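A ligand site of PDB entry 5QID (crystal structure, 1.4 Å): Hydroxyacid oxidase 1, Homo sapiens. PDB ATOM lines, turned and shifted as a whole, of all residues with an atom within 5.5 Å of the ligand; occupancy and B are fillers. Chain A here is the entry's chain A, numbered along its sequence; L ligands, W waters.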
ATOM      1  N   TYR A  27     -36.669  -1.167  -0.666  1.00  0.00           N
ATOM      2  CA  TYR A  27     -35.503  -0.652  -1.333  1.00  0.00           C
ATOM      3  C   TYR A  27     -35.080  -1.645  -2.453  1.00  0.00           C
ATOM      4  O   TYR A  27     -34.765  -1.220  -3.575  1.00  0.00           O
ATOM      5  CB  TYR A  27     -34.338  -0.333  -0.352  1.00  0.00           C
ATOM      6  CG  TYR A  27     -33.052  -0.101  -1.073  1.00  0.00           C
ATOM      7  CD1 TYR A  27     -32.819   1.037  -1.848  1.00  0.00           C
ATOM      8  CD2 TYR A  27     -32.077  -1.121  -1.142  1.00  0.00           C
ATOM      9  CE1 TYR A  27     -31.660   1.181  -2.612  1.00  0.00           C
ATOM     10  CE2 TYR A  27     -30.921  -0.965  -1.884  1.00  0.00           C
ATOM     11  CZ  TYR A  27     -30.690   0.167  -2.586  1.00  0.00           C
ATOM     12  OH  TYR A  27     -29.607   0.286  -3.400  1.00  0.00           O
ATOM     13  N   TYR A  28     -35.026  -2.923  -2.104  1.00  0.00           N
ATOM     14  CA  TYR A  28     -34.514  -3.939  -3.014  1.00  0.00           C
ATOM     15  C   TYR A  28     -35.564  -4.213  -4.099  1.00  0.00           C
ATOM     16  O   TYR A  28     -35.156  -4.410  -5.277  1.00  0.00           O
ATOM     17  CB  TYR A  28     -34.208  -5.197  -2.256  1.00  0.00           C
ATOM     18  CG  TYR A  28     -33.021  -5.181  -1.300  1.00  0.00           C
ATOM     19  CD1 TYR A  28     -31.794  -4.732  -1.687  1.00  0.00           C
ATOM     20  CD2 TYR A  28     -33.135  -5.789  -0.032  1.00  0.00           C
ATOM     21  CE1 TYR A  28     -30.657  -4.786  -0.809  1.00  0.00           C
ATOM     22  CE2 TYR A  28     -32.016  -5.856   0.817  1.00  0.00           C
ATOM     23  CZ  TYR A  28     -30.818  -5.335   0.395  1.00  0.00           C
ATOM     24  OH  TYR A  28     -29.652  -5.417   1.153  1.00  0.00           O
ATOM     25  N   SER A  30     -38.113  -2.351  -5.316  1.00  0.00           N
ATOM     26  CA  SER A  30     -38.769  -1.289  -6.025  1.00  0.00           C
ATOM     27  C   SER A  30     -38.229  -1.036  -7.406  1.00  0.00           C
ATOM     28  O   SER A  30     -37.051  -1.253  -7.681  1.00  0.00           O
ATOM     29  CB  SER A  30     -38.618   0.026  -5.236  1.00  0.00           C
ATOM     30  OG  SER A  30     -39.676   0.031  -4.368  1.00  0.00           O
ATOM     31  N   ASN A  41     -40.105  -6.229 -17.510  1.00  0.00           N
ATOM     32  CA  ASN A  41     -38.903  -7.047 -17.553  1.00  0.00           C
ATOM     33  C   ASN A  41     -39.188  -8.512 -17.373  1.00  0.00           C
ATOM     34  O   ASN A  41     -38.549  -9.364 -18.052  1.00  0.00           O
ATOM     35  CB  ASN A  41     -37.873  -6.624 -16.491  1.00  0.00           C
ATOM     36  CG  ASN A  41     -37.020  -5.455 -16.888  1.00  0.00           C
ATOM     37  OD1 ASN A  41     -37.057  -5.018 -18.078  1.00  0.00           O
ATOM     38  ND2 ASN A  41     -36.286  -4.888 -15.924  1.00  0.00           N
ATOM     39  N   GLY A  79     -24.905  -9.712 -10.822  1.00  0.00           N
ATOM     40  CA  GLY A  79     -24.858  -8.287 -11.089  1.00  0.00           C
ATOM     41  C   GLY A  79     -24.673  -7.455  -9.850  1.00  0.00           C
ATOM     42  O   GLY A  79     -24.939  -7.900  -8.756  1.00  0.00           O
ATOM     43  N   ALA A  80     -24.238  -6.193 -10.032  1.00  0.00           N
ATOM     44  CA  ALA A  80     -23.971  -5.244  -8.923  1.00  0.00           C
ATOM     45  C   ALA A  80     -25.276  -4.854  -8.237  1.00  0.00           C
ATOM     46  O   ALA A  80     -26.212  -4.344  -8.922  1.00  0.00           O
ATOM     47  CB  ALA A  80     -23.247  -4.024  -9.476  1.00  0.00           C
ATOM     48  N   THR A  81     -25.384  -5.099  -6.950  1.00  0.00           N
ATOM     49  CA  THR A  81     -26.499  -4.615  -6.168  1.00  0.00           C
ATOM     50  C   THR A  81     -25.905  -3.967  -4.956  1.00  0.00           C
ATOM     51  O   THR A  81     -25.049  -4.592  -4.268  1.00  0.00           O
ATOM     52  CB  THR A  81     -27.514  -5.669  -5.761  1.00  0.00           C
ATOM     53  OG1 THR A  81     -26.836  -6.820  -5.277  1.00  0.00           O
ATOM     54  CG2 THR A  81     -28.354  -6.132  -6.953  1.00  0.00           C
ATOM     55  N   ALA A  82     -26.255  -2.733  -4.700  1.00  0.00           N
ATOM     56  CA  ALA A  82     -25.670  -1.975  -3.628  1.00  0.00           C
ATOM     57  C   ALA A  82     -26.052  -2.520  -2.255  1.00  0.00           C
ATOM     58  O   ALA A  82     -27.106  -3.106  -2.056  1.00  0.00           O
ATOM     59  CB  ALA A  82     -26.114  -0.503  -3.709  1.00  0.00           C
ATOM     60  N   MET A 107     -19.953  -9.158 -10.151  1.00  0.00           N
ATOM     61  CA  MET A 107     -19.804  -7.733 -10.425  1.00  0.00           C
ATOM     62  C   MET A 107     -20.065  -6.986  -9.095  1.00  0.00           C
ATOM     63  O   MET A 107     -21.153  -7.017  -8.550  1.00  0.00           O
ATOM     64  CB  MET A 107     -20.829  -7.309 -11.491  1.00  0.00           C
ATOM     65  CG  MET A 107     -20.599  -5.891 -11.982  1.00  0.00           C
ATOM     66  SD  MET A 107     -22.047  -5.128 -12.764  1.00  0.00           S
ATOM     67  CE  MET A 107     -22.406  -6.321 -14.070  1.00  0.00           C
ATOM     68  N   SER A 109     -20.548  -3.768  -6.789  1.00  0.00           N
ATOM     69  CA  SER A 109     -21.047  -2.380  -6.823  1.00  0.00           C
ATOM     70  C   SER A 109     -20.014  -1.388  -6.369  1.00  0.00           C
ATOM     71  O   SER A 109     -19.366  -1.626  -5.329  1.00  0.00           O
ATOM     72  CB  SER A 109     -22.241  -2.310  -5.900  1.00  0.00           C
ATOM     73  OG  SER A 109     -22.744  -0.962  -5.834  1.00  0.00           O
ATOM     74  N   SER A 110     -20.006  -0.226  -6.996  1.00  0.00           N
ATOM     75  CA  SER A 110     -19.277   0.928  -6.407  1.00  0.00           C
ATOM     76  C   SER A 110     -19.849   1.352  -5.017  1.00  0.00           C
ATOM     77  O   SER A 110     -19.113   1.985  -4.215  1.00  0.00           O
ATOM     78  CB  SER A 110     -19.286   2.151  -7.385  1.00  0.00           C
ATOM     79  OG  SER A 110     -18.210   2.059  -8.319  1.00  0.00           O
ATOM     80  N   TRP A 111     -21.103   0.991  -4.757  1.00  0.00           N
ATOM     81  CA  TRP A 111     -21.860   1.318  -3.527  1.00  0.00           C
ATOM     82  C   TRP A 111     -22.044   0.107  -2.582  1.00  0.00           C
ATOM     83  O   TRP A 111     -23.054  -0.002  -1.870  1.00  0.00           O
ATOM     84  CB  TRP A 111     -23.248   1.854  -3.876  1.00  0.00           C
ATOM     85  CG  TRP A 111     -23.256   3.115  -4.701  1.00  0.00           C
ATOM     86  CD1 TRP A 111     -22.229   3.979  -4.858  1.00  0.00           C
ATOM     87  CD2 TRP A 111     -24.358   3.662  -5.461  1.00  0.00           C
ATOM     88  NE1 TRP A 111     -22.591   5.026  -5.680  1.00  0.00           N
ATOM     89  CE2 TRP A 111     -23.906   4.863  -6.047  1.00  0.00           C
ATOM     90  CE3 TRP A 111     -25.681   3.266  -5.675  1.00  0.00           C
ATOM     91  CZ2 TRP A 111     -24.725   5.649  -6.853  1.00  0.00           C
ATOM     92  CZ3 TRP A 111     -26.482   4.073  -6.494  1.00  0.00           C
ATOM     93  CH2 TRP A 111     -25.995   5.225  -7.063  1.00  0.00           C
ATOM     94  N   GLN A 131     -18.130  -2.711 -10.900  1.00  0.00           N
ATOM     95  CA  GLN A 131     -19.089  -1.717 -11.466  1.00  0.00           C
ATOM     96  C   GLN A 131     -18.670  -0.344 -10.961  1.00  0.00           C
ATOM     97  O   GLN A 131     -18.517  -0.146  -9.759  1.00  0.00           O
ATOM     98  CB  GLN A 131     -20.485  -2.039 -11.039  1.00  0.00           C
ATOM     99  CG  GLN A 131     -21.560  -1.030 -11.463  1.00  0.00           C
ATOM    100  CD  GLN A 131     -21.665   0.132 -10.491  1.00  0.00           C
ATOM    101  OE1 GLN A 131     -21.867  -0.130  -9.313  1.00  0.00           O
ATOM    102  NE2 GLN A 131     -21.726   1.392 -11.005  1.00  0.00           N
ATOM    103  N   TYR A 133     -19.176   3.937 -11.049  1.00  0.00           N
ATOM    104  CA  TYR A 133     -19.846   5.169 -11.340  1.00  0.00           C
ATOM    105  C   TYR A 133     -18.744   6.222 -11.536  1.00  0.00           C
ATOM    106  O   TYR A 133     -17.702   6.181 -10.807  1.00  0.00           O
ATOM    107  CB  TYR A 133     -20.727   5.580 -10.176  1.00  0.00           C
ATOM    108  CG  TYR A 133     -22.061   4.878 -10.119  1.00  0.00           C
ATOM    109  CD1 TYR A 133     -22.924   5.027 -11.168  1.00  0.00           C
ATOM    110  CD2 TYR A 133     -22.438   4.075  -9.070  1.00  0.00           C
ATOM    111  CE1 TYR A 133     -24.124   4.385 -11.164  1.00  0.00           C
ATOM    112  CE2 TYR A 133     -23.674   3.425  -9.058  1.00  0.00           C
ATOM    113  CZ  TYR A 133     -24.520   3.653 -10.114  1.00  0.00           C
ATOM    114  OH  TYR A 133     -25.757   3.020 -10.154  1.00  0.00           O
ATOM    115  N   THR A 159     -21.409   2.223 -15.412  1.00  0.00           N
ATOM    116  CA  THR A 159     -22.881   2.437 -15.475  1.00  0.00           C
ATOM    117  C   THR A 159     -23.103   3.778 -16.110  1.00  0.00           C
ATOM    118  O   THR A 159     -22.517   4.816 -15.635  1.00  0.00           O
ATOM    119  CB  THR A 159     -23.486   2.322 -14.080  1.00  0.00           C
ATOM    120  OG1 THR A 159     -23.220   1.017 -13.574  1.00  0.00           O
ATOM    121  CG2 THR A 159     -24.961   2.567 -14.150  1.00  0.00           C
ATOM    122  N   LYS A 237     -22.671  -0.331 -19.231  1.00  0.00           N
ATOM    123  CA  LYS A 237     -23.833  -0.903 -18.579  1.00  0.00           C
ATOM    124  C   LYS A 237     -24.988   0.114 -18.551  1.00  0.00           C
ATOM    125  O   LYS A 237     -24.852   1.203 -17.994  1.00  0.00           O
ATOM    126  CB  LYS A 237     -23.449  -1.366 -17.198  1.00  0.00           C
ATOM    127  CG  LYS A 237     -24.615  -1.780 -16.317  1.00  0.00           C
ATOM    128  CD  LYS A 237     -24.148  -2.193 -14.912  1.00  0.00           C
ATOM    129  CE  LYS A 237     -25.219  -2.805 -13.998  1.00  0.00           C
ATOM    130  NZ  LYS A 237     -26.174  -1.829 -13.522  1.00  0.00           N
ATOM    131  N   SER A 259     -29.365  -3.139 -20.228  1.00  0.00           N
ATOM    132  CA  SER A 259     -29.845  -3.037 -18.884  1.00  0.00           C
ATOM    133  C   SER A 259     -30.703  -1.798 -18.793  1.00  0.00           C
ATOM    134  O   SER A 259     -30.368  -0.772 -19.407  1.00  0.00           O
ATOM    135  CB  SER A 259     -28.667  -2.887 -17.927  1.00  0.00           C
ATOM    136  OG  SER A 259     -29.114  -2.730 -16.565  1.00  0.00           O
ATOM    137  N   HIS A 261     -31.336  -0.990 -15.596  1.00  0.00           N
ATOM    138  CA  HIS A 261     -30.994  -0.767 -14.166  1.00  0.00           C
ATOM    139  C   HIS A 261     -32.047  -1.416 -13.271  1.00  0.00           C
ATOM    140  O   HIS A 261     -32.457  -0.874 -12.238  1.00  0.00           O
ATOM    141  CB  HIS A 261     -30.805   0.729 -13.918  1.00  0.00           C
ATOM    142  CG  HIS A 261     -29.930   1.082 -12.768  1.00  0.00           C
ATOM    143  ND1 HIS A 261     -28.797   1.866 -12.940  1.00  0.00           N
ATOM    144  CD2 HIS A 261     -30.040   0.864 -11.425  1.00  0.00           C
ATOM    145  CE1 HIS A 261     -28.247   2.071 -11.748  1.00  0.00           C
ATOM    146  NE2 HIS A 261     -28.978   1.495 -10.808  1.00  0.00           N
ATOM    147  N   GLY A 262     -32.528  -2.603 -13.629  1.00  0.00           N
ATOM    148  CA  GLY A 262     -33.540  -3.321 -12.855  1.00  0.00           C
ATOM    149  C   GLY A 262     -34.838  -2.499 -12.792  1.00  0.00           C
ATOM    150  O   GLY A 262     -35.602  -2.619 -11.846  1.00  0.00           O
ATOM    151  N   ARG A 264     -35.197   0.648 -12.429  1.00  0.00           N
ATOM    152  CA  ARG A 264     -35.129   1.587 -11.305  1.00  0.00           C
ATOM    153  C   ARG A 264     -34.782   2.996 -11.735  1.00  0.00           C
ATOM    154  O   ARG A 264     -34.668   3.895 -10.843  1.00  0.00           O
ATOM    155  CB  ARG A 264     -34.082   1.093 -10.250  1.00  0.00           C
ATOM    156  CG  ARG A 264     -34.472  -0.205  -9.610  1.00  0.00           C
ATOM    157  CD  ARG A 264     -33.342  -0.931  -8.955  1.00  0.00           C
ATOM    158  NE  ARG A 264     -32.849  -0.341  -7.742  1.00  0.00           N
ATOM    159  CZ  ARG A 264     -33.383  -0.548  -6.534  1.00  0.00           C
ATOM    160  NH1 ARG A 264     -34.469  -1.247  -6.358  1.00  0.00           N
ATOM    161  NH2 ARG A 264     -32.752  -0.085  -5.436  1.00  0.00           N
ATOM    162  N   ASP A 292     -29.271  -7.923 -18.369  1.00  0.00           N
ATOM    163  CA  ASP A 292     -29.852  -8.109 -17.016  1.00  0.00           C
ATOM    164  C   ASP A 292     -31.252  -7.494 -17.064  1.00  0.00           C
ATOM    165  O   ASP A 292     -31.641  -6.809 -18.008  1.00  0.00           O
ATOM    166  CB  ASP A 292     -28.968  -7.543 -15.872  1.00  0.00           C
ATOM    167  CG  ASP A 292     -28.821  -6.093 -15.846  1.00  0.00           C
ATOM    168  OD1 ASP A 292     -29.667  -5.315 -16.333  1.00  0.00           O
ATOM    169  OD2 ASP A 292     -27.813  -5.609 -15.242  1.00  0.00           O
ATOM    170  N   GLY A 293     -32.026  -7.785 -16.023  1.00  0.00           N
ATOM    171  CA  GLY A 293     -33.377  -7.262 -15.872  1.00  0.00           C
ATOM    172  C   GLY A 293     -34.417  -8.384 -16.055  1.00  0.00           C
ATOM    173  O   GLY A 293     -34.747  -8.721 -17.164  1.00  0.00           O
ATOM    174  N   GLY A 294     -34.952  -8.877 -14.932  1.00  0.00           N
ATOM    175  CA  GLY A 294     -36.023  -9.822 -15.001  1.00  0.00           C
ATOM    176  C   GLY A 294     -35.655 -11.276 -15.125  1.00  0.00           C
ATOM    177  O   GLY A 294     -36.543 -12.099 -15.277  1.00  0.00           O
ATOM    178  N   VAL A 295     -34.380 -11.612 -15.038  1.00  0.00           N
ATOM    179  CA  VAL A 295     -33.963 -13.011 -15.118  1.00  0.00           C
ATOM    180  C   VAL A 295     -34.304 -13.697 -13.789  1.00  0.00           C
ATOM    181  O   VAL A 295     -33.746 -13.348 -12.707  1.00  0.00           O
ATOM    182  CB  VAL A 295     -32.447 -13.167 -15.460  1.00  0.00           C
ATOM    183  CG1 VAL A 295     -32.021 -14.615 -15.372  1.00  0.00           C
ATOM    184  CG2 VAL A 295     -32.148 -12.541 -16.811  1.00  0.00           C
ATOM    185  N   ARG A 296     -35.190 -14.698 -13.863  1.00  0.00           N
ATOM    186  CA  ARG A 296     -35.643 -15.438 -12.664  1.00  0.00           C
ATOM    187  C   ARG A 296     -35.650 -16.940 -12.860  1.00  0.00           C
ATOM    188  O   ARG A 296     -35.744 -17.655 -11.873  1.00  0.00           O
ATOM    189  CB  ARG A 296     -37.042 -15.029 -12.318  1.00  0.00           C
ATOM    190  CG  ARG A 296     -37.292 -13.535 -12.117  1.00  0.00           C
ATOM    191  CD  ARG A 296     -36.638 -12.998 -10.853  1.00  0.00           C
ATOM    192  NE  ARG A 296     -36.840 -11.530 -10.733  1.00  0.00           N
ATOM    193  CZ  ARG A 296     -35.962 -10.608 -11.096  1.00  0.00           C
ATOM    194  NH1 ARG A 296     -34.753 -10.922 -11.604  1.00  0.00           N
ATOM    195  NH2 ARG A 296     -36.230  -9.307 -10.868  1.00  0.00           N
ATOM    196  N   PHE A 313     -26.891 -11.405 -16.237  1.00  0.00           N
ATOM    197  CA  PHE A 313     -26.603 -11.043 -14.853  1.00  0.00           C
ATOM    198  C   PHE A 313     -27.911 -11.042 -14.094  1.00  0.00           C
ATOM    199  O   PHE A 313     -28.947 -10.643 -14.613  1.00  0.00           O
ATOM    200  CB  PHE A 313     -25.898  -9.679 -14.728  1.00  0.00           C
ATOM    201  CG  PHE A 313     -24.519  -9.683 -15.324  1.00  0.00           C
ATOM    202  CD1 PHE A 313     -23.426  -9.828 -14.535  1.00  0.00           C
ATOM    203  CD2 PHE A 313     -24.330  -9.606 -16.676  1.00  0.00           C
ATOM    204  CE1 PHE A 313     -22.153  -9.876 -15.077  1.00  0.00           C
ATOM    205  CE2 PHE A 313     -23.083  -9.705 -17.233  1.00  0.00           C
ATOM    206  CZ  PHE A 313     -21.967  -9.823 -16.422  1.00  0.00           C
ATOM    207  N   VAL A 314     -27.817 -11.403 -12.823  1.00  0.00           N
ATOM    208  CA  VAL A 314     -28.945 -11.410 -11.886  1.00  0.00           C
ATOM    209  C   VAL A 314     -28.699 -10.462 -10.784  1.00  0.00           C
ATOM    210  O   VAL A 314     -27.604 -10.485 -10.182  1.00  0.00           O
ATOM    211  CB  VAL A 314     -29.354 -12.774 -11.344  1.00  0.00           C
ATOM    212  CG1 VAL A 314     -30.130 -13.540 -12.451  1.00  0.00           C
ATOM    213  CG2 VAL A 314     -28.228 -13.533 -10.780  1.00  0.00           C
ATOM    214  N   GLY A 315     -29.697  -9.632 -10.498  1.00  0.00           N
ATOM    215  CA  GLY A 315     -29.607  -8.661  -9.415  1.00  0.00           C
ATOM    216  C   GLY A 315     -30.377  -9.105  -8.187  1.00  0.00           C
ATOM    217  O   GLY A 315     -29.787  -9.700  -7.260  1.00  0.00           O
ATOM    218  N   ARG A 316     -31.671  -8.861  -8.153  1.00  0.00           N
ATOM    219  CA  ARG A 316     -32.465  -9.103  -6.954  1.00  0.00           C
ATOM    220  C   ARG A 316     -32.386 -10.527  -6.452  1.00  0.00           C
ATOM    221  O   ARG A 316     -32.320 -10.679  -5.243  1.00  0.00           O
ATOM    222  CB  ARG A 316     -33.914  -8.694  -7.179  1.00  0.00           C
ATOM    223  CG  ARG A 316     -34.089  -7.200  -7.313  1.00  0.00           C
ATOM    224  CD  ARG A 316     -35.499  -6.837  -7.657  1.00  0.00           C
ATOM    225  NE  ARG A 316     -35.691  -5.385  -7.897  1.00  0.00           N
ATOM    226  CZ  ARG A 316     -35.594  -4.776  -9.064  1.00  0.00           C
ATOM    227  NH1 ARG A 316     -35.265  -5.461 -10.141  1.00  0.00           N
ATOM    228  NH2 ARG A 316     -35.938  -3.489  -9.141  1.00  0.00           N
ATOM    229  N   PRO A 317     -32.392 -11.545  -7.308  1.00  0.00           N
ATOM    230  CA  PRO A 317     -32.381 -12.959  -6.776  1.00  0.00           C
ATOM    231  C   PRO A 317     -31.206 -13.166  -5.794  1.00  0.00           C
ATOM    232  O   PRO A 317     -31.363 -13.905  -4.800  1.00  0.00           O
ATOM    233  CB  PRO A 317     -32.263 -13.767  -8.003  1.00  0.00           C
ATOM    234  CG  PRO A 317     -33.077 -12.963  -9.028  1.00  0.00           C
ATOM    235  CD  PRO A 317     -32.608 -11.561  -8.779  1.00  0.00           C
ATOM    236  N   VAL A 319     -29.799 -10.947  -3.759  1.00  0.00           N
ATOM    237  CA  VAL A 319     -30.166 -10.302  -2.498  1.00  0.00           C
ATOM    238  C   VAL A 319     -31.134 -11.171  -1.757  1.00  0.00           C
ATOM    239  O   VAL A 319     -31.022 -11.328  -0.501  1.00  0.00           O
ATOM    240  CB  VAL A 319     -30.775  -8.906  -2.761  1.00  0.00           C
ATOM    241  CG1 VAL A 319     -31.272  -8.318  -1.434  1.00  0.00           C
ATOM    242  CG2 VAL A 319     -29.768  -8.023  -3.466  1.00  0.00           C
HETATM  243  N1  LIG L   1     -26.557  -1.094 -10.672  1.00  0.00           N
HETATM  244  C1  LIG L   1     -25.349  -0.496 -10.571  1.00  0.00           C
HETATM  245  O1  LIG L   1     -24.765  -0.186 -11.601  1.00  0.00           O
HETATM  246  N2  LIG L   1     -24.826  -0.236  -9.362  1.00  0.00           N
HETATM  247  C2  LIG L   1     -25.454  -0.422  -8.227  1.00  0.00           C
HETATM  248  O2  LIG L   1     -24.931  -0.172  -7.125  1.00  0.00           O
HETATM  249  C3  LIG L   1     -26.763  -1.046  -8.227  1.00  0.00           C
HETATM  250  N3  LIG L   1     -27.456  -1.328  -7.093  1.00  0.00           N
HETATM  251  C4  LIG L   1     -28.659  -1.943  -7.151  1.00  0.00           C
HETATM  252  C5  LIG L   1     -29.350  -2.255  -5.978  1.00  0.00           C
HETATM  253  C6  LIG L   1     -30.562  -2.887  -6.051  1.00  0.00           C
HETATM  254  C7  LIG L   1     -31.314  -3.228  -4.806  1.00  0.00           C
HETATM  255  C8  LIG L   1     -31.079  -3.304  -7.371  1.00  0.00           C
HETATM  256  C9  LIG L   1     -32.399  -4.070  -7.465  1.00  0.00           C
HETATM  257  C10 LIG L   1     -30.388  -3.061  -8.531  1.00  0.00           C
HETATM  258  C11 LIG L   1     -29.204  -2.330  -8.478  1.00  0.00           C
HETATM  259  N4  LIG L   1     -28.462  -2.056  -9.628  1.00  0.00           N
HETATM  260  C12 LIG L   1     -27.254  -1.344  -9.547  1.00  0.00           C
HETATM  261  C13 LIG L   1     -28.882  -2.490 -10.979  1.00  0.00           C
HETATM  262  C14 LIG L   1     -28.406  -3.960 -11.068  1.00  0.00           C
HETATM  263  O3  LIG L   1     -26.990  -3.999 -11.400  1.00  0.00           O
HETATM  264  C15 LIG L   1     -29.040  -4.740 -12.202  1.00  0.00           C
HETATM  265  O4  LIG L   1     -29.024  -3.918 -13.427  1.00  0.00           O
HETATM  266  C16 LIG L   1     -30.458  -5.105 -11.988  1.00  0.00           C
HETATM  267  O5  LIG L   1     -30.637  -5.542 -10.576  1.00  0.00           O
HETATM  268  C17 LIG L   1     -30.925  -6.195 -12.885  1.00  0.00           C
HETATM  269  O6  LIG L   1     -32.288  -6.628 -12.734  1.00  0.00           O
HETATM  270  P1  LIG L   1     -32.877  -7.790 -11.755  1.00  0.00           P
HETATM  271  O7  LIG L   1     -32.067  -9.056 -11.843  1.00  0.00           O
HETATM  272  O8  LIG L   1     -34.274  -7.911 -12.284  1.00  0.00           O
HETATM  273  O9  LIG L   1     -32.844  -7.259 -10.335  1.00  0.00           O
HETATM  274  O   HOH W   1     -35.897  -5.825 -13.187  1.00  0.00           O
HETATM  275  O   HOH W   2     -31.700 -10.022 -14.341  1.00  0.00           O
HETATM  276  O   HOH W   3     -25.928  -6.110 -13.195  1.00  0.00           O
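The backbone NH (N) of Ala 82 sits at hydrogen-bond distance from a nitrogen (N3) of the ligand (3.0 Å).
The backbone carbonyl oxygen (O) of Ala 80 sits at hydrogen-bond distance from an oxygen (O3) of the ligand, 2.6 Å away.
O4 of the ligand is in hydrogen-bond range of OG of Ser 259 (3.4 Å).
The backbone NH (N) of Arg 316 is in hydrogen-bond range of an oxygen (O9) of the ligand, at 3.0 Å.
N2 of the ligand is in hydrogen-bond range of OE1 of Gln 131 (3.0 Å).
O2 of the ligand is in hydrogen-bond range of OG of Ser 109, at 2.7 Å.
The side-chain carboxylate (OD2) of Asp 292 lies within hydrogen-bond range of an oxygen (O4) of the ligand, at 2.8 Å.
The guanidinium group of Arg 316 lies within salt-bridge range of an oxygen (O9) of the ligand, 3.0 Å away.
O7 of the ligand lies within hydrogen-bond range of N of Gly 315 (2.8 Å).
An oxygen (O8) of the ligand is in hydrogen-bond range of the backbone NH (N) of Gly 294.
The side-chain hydroxyl (OG1) of Thr 159 is in hydrogen-bond range of an oxygen (O1) of the ligand (2.8 Å).
The backbone NH (N) of Gly 293 sits close to an oxygen (O6) of the ligand.
NZ of Lys 237 lies within hydrogen-bond range of O1 of the ligand.
N2 of the ligand lies within hydrogen-bond range of OH of Tyr 133.
An oxygen (O8) of the ligand lies within salt-bridge range of the guanidinium group of Arg 296 (2.8 Å).
The guanidinium group (NH1) of Arg 264 lies within hydrogen-bond range of the backbone carbonyl oxygen (O) of Tyr 27, 2.8 Å away.
The backbone carbonyl oxygen of Gln 131 sits at hydrogen-bond distance from the side-chain hydroxyl of Ser 110, 2.7 Å away.
NE2 of Gln 131 lies within hydrogen-bond range of OG1 of Thr 159.
The side-chain hydroxyl of Ser 259 lies within hydrogen-bond range of the side-chain carboxylate of Asp 292, at 2.7 Å.
The side-chain hydroxyl (OG) of Ser 109 is in hydrogen-bond range of the backbone NH (N) of Trp 111, at 2.8 Å.
N of Gly 79 lies within hydrogen-bond range of O of Val 314 (2.9 Å).
The guanidinium group (NH1) of Arg 264 is in hydrogen-bond range of the backbone carbonyl oxygen (O) of Tyr 28, at 3.4 Å.
O of Ser 30 lies within hydrogen-bond range of NH1 of Arg 264 (2.9 Å).
Residues that only touch the ligand: Arg 264 (3.5 Å), Tyr 28 (3.5 Å), Gly 262 (3.5 Å), Thr 81 (3.5 Å), His 261 (3.5 Å), Tyr 27 (3.6 Å), Val 314 (3.8 Å), Trp 111 (3.8 Å) and Pro 317 (3.99 Å).
Hydrophobic or aromatic side chains within 4 Å of the ligand: Tyr 27, Tyr 28, Ala 82, Trp 111, Tyr 133, His 261 and Pro 317.
The nearest printed residue that does not touch the ligand is Gly 79 (4.4 Å).
Water W1 lies within hydrogen-bond range of O8 of the ligand, ND2 of Asn 41, NH1 of Arg 316 and O of Gly 262.
Water W3 lies within hydrogen-bond range of the side-chain carboxylate (OD2) of Asp 292 (2.8 Å) and an oxygen (O3) of the ligand (3.0 Å).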
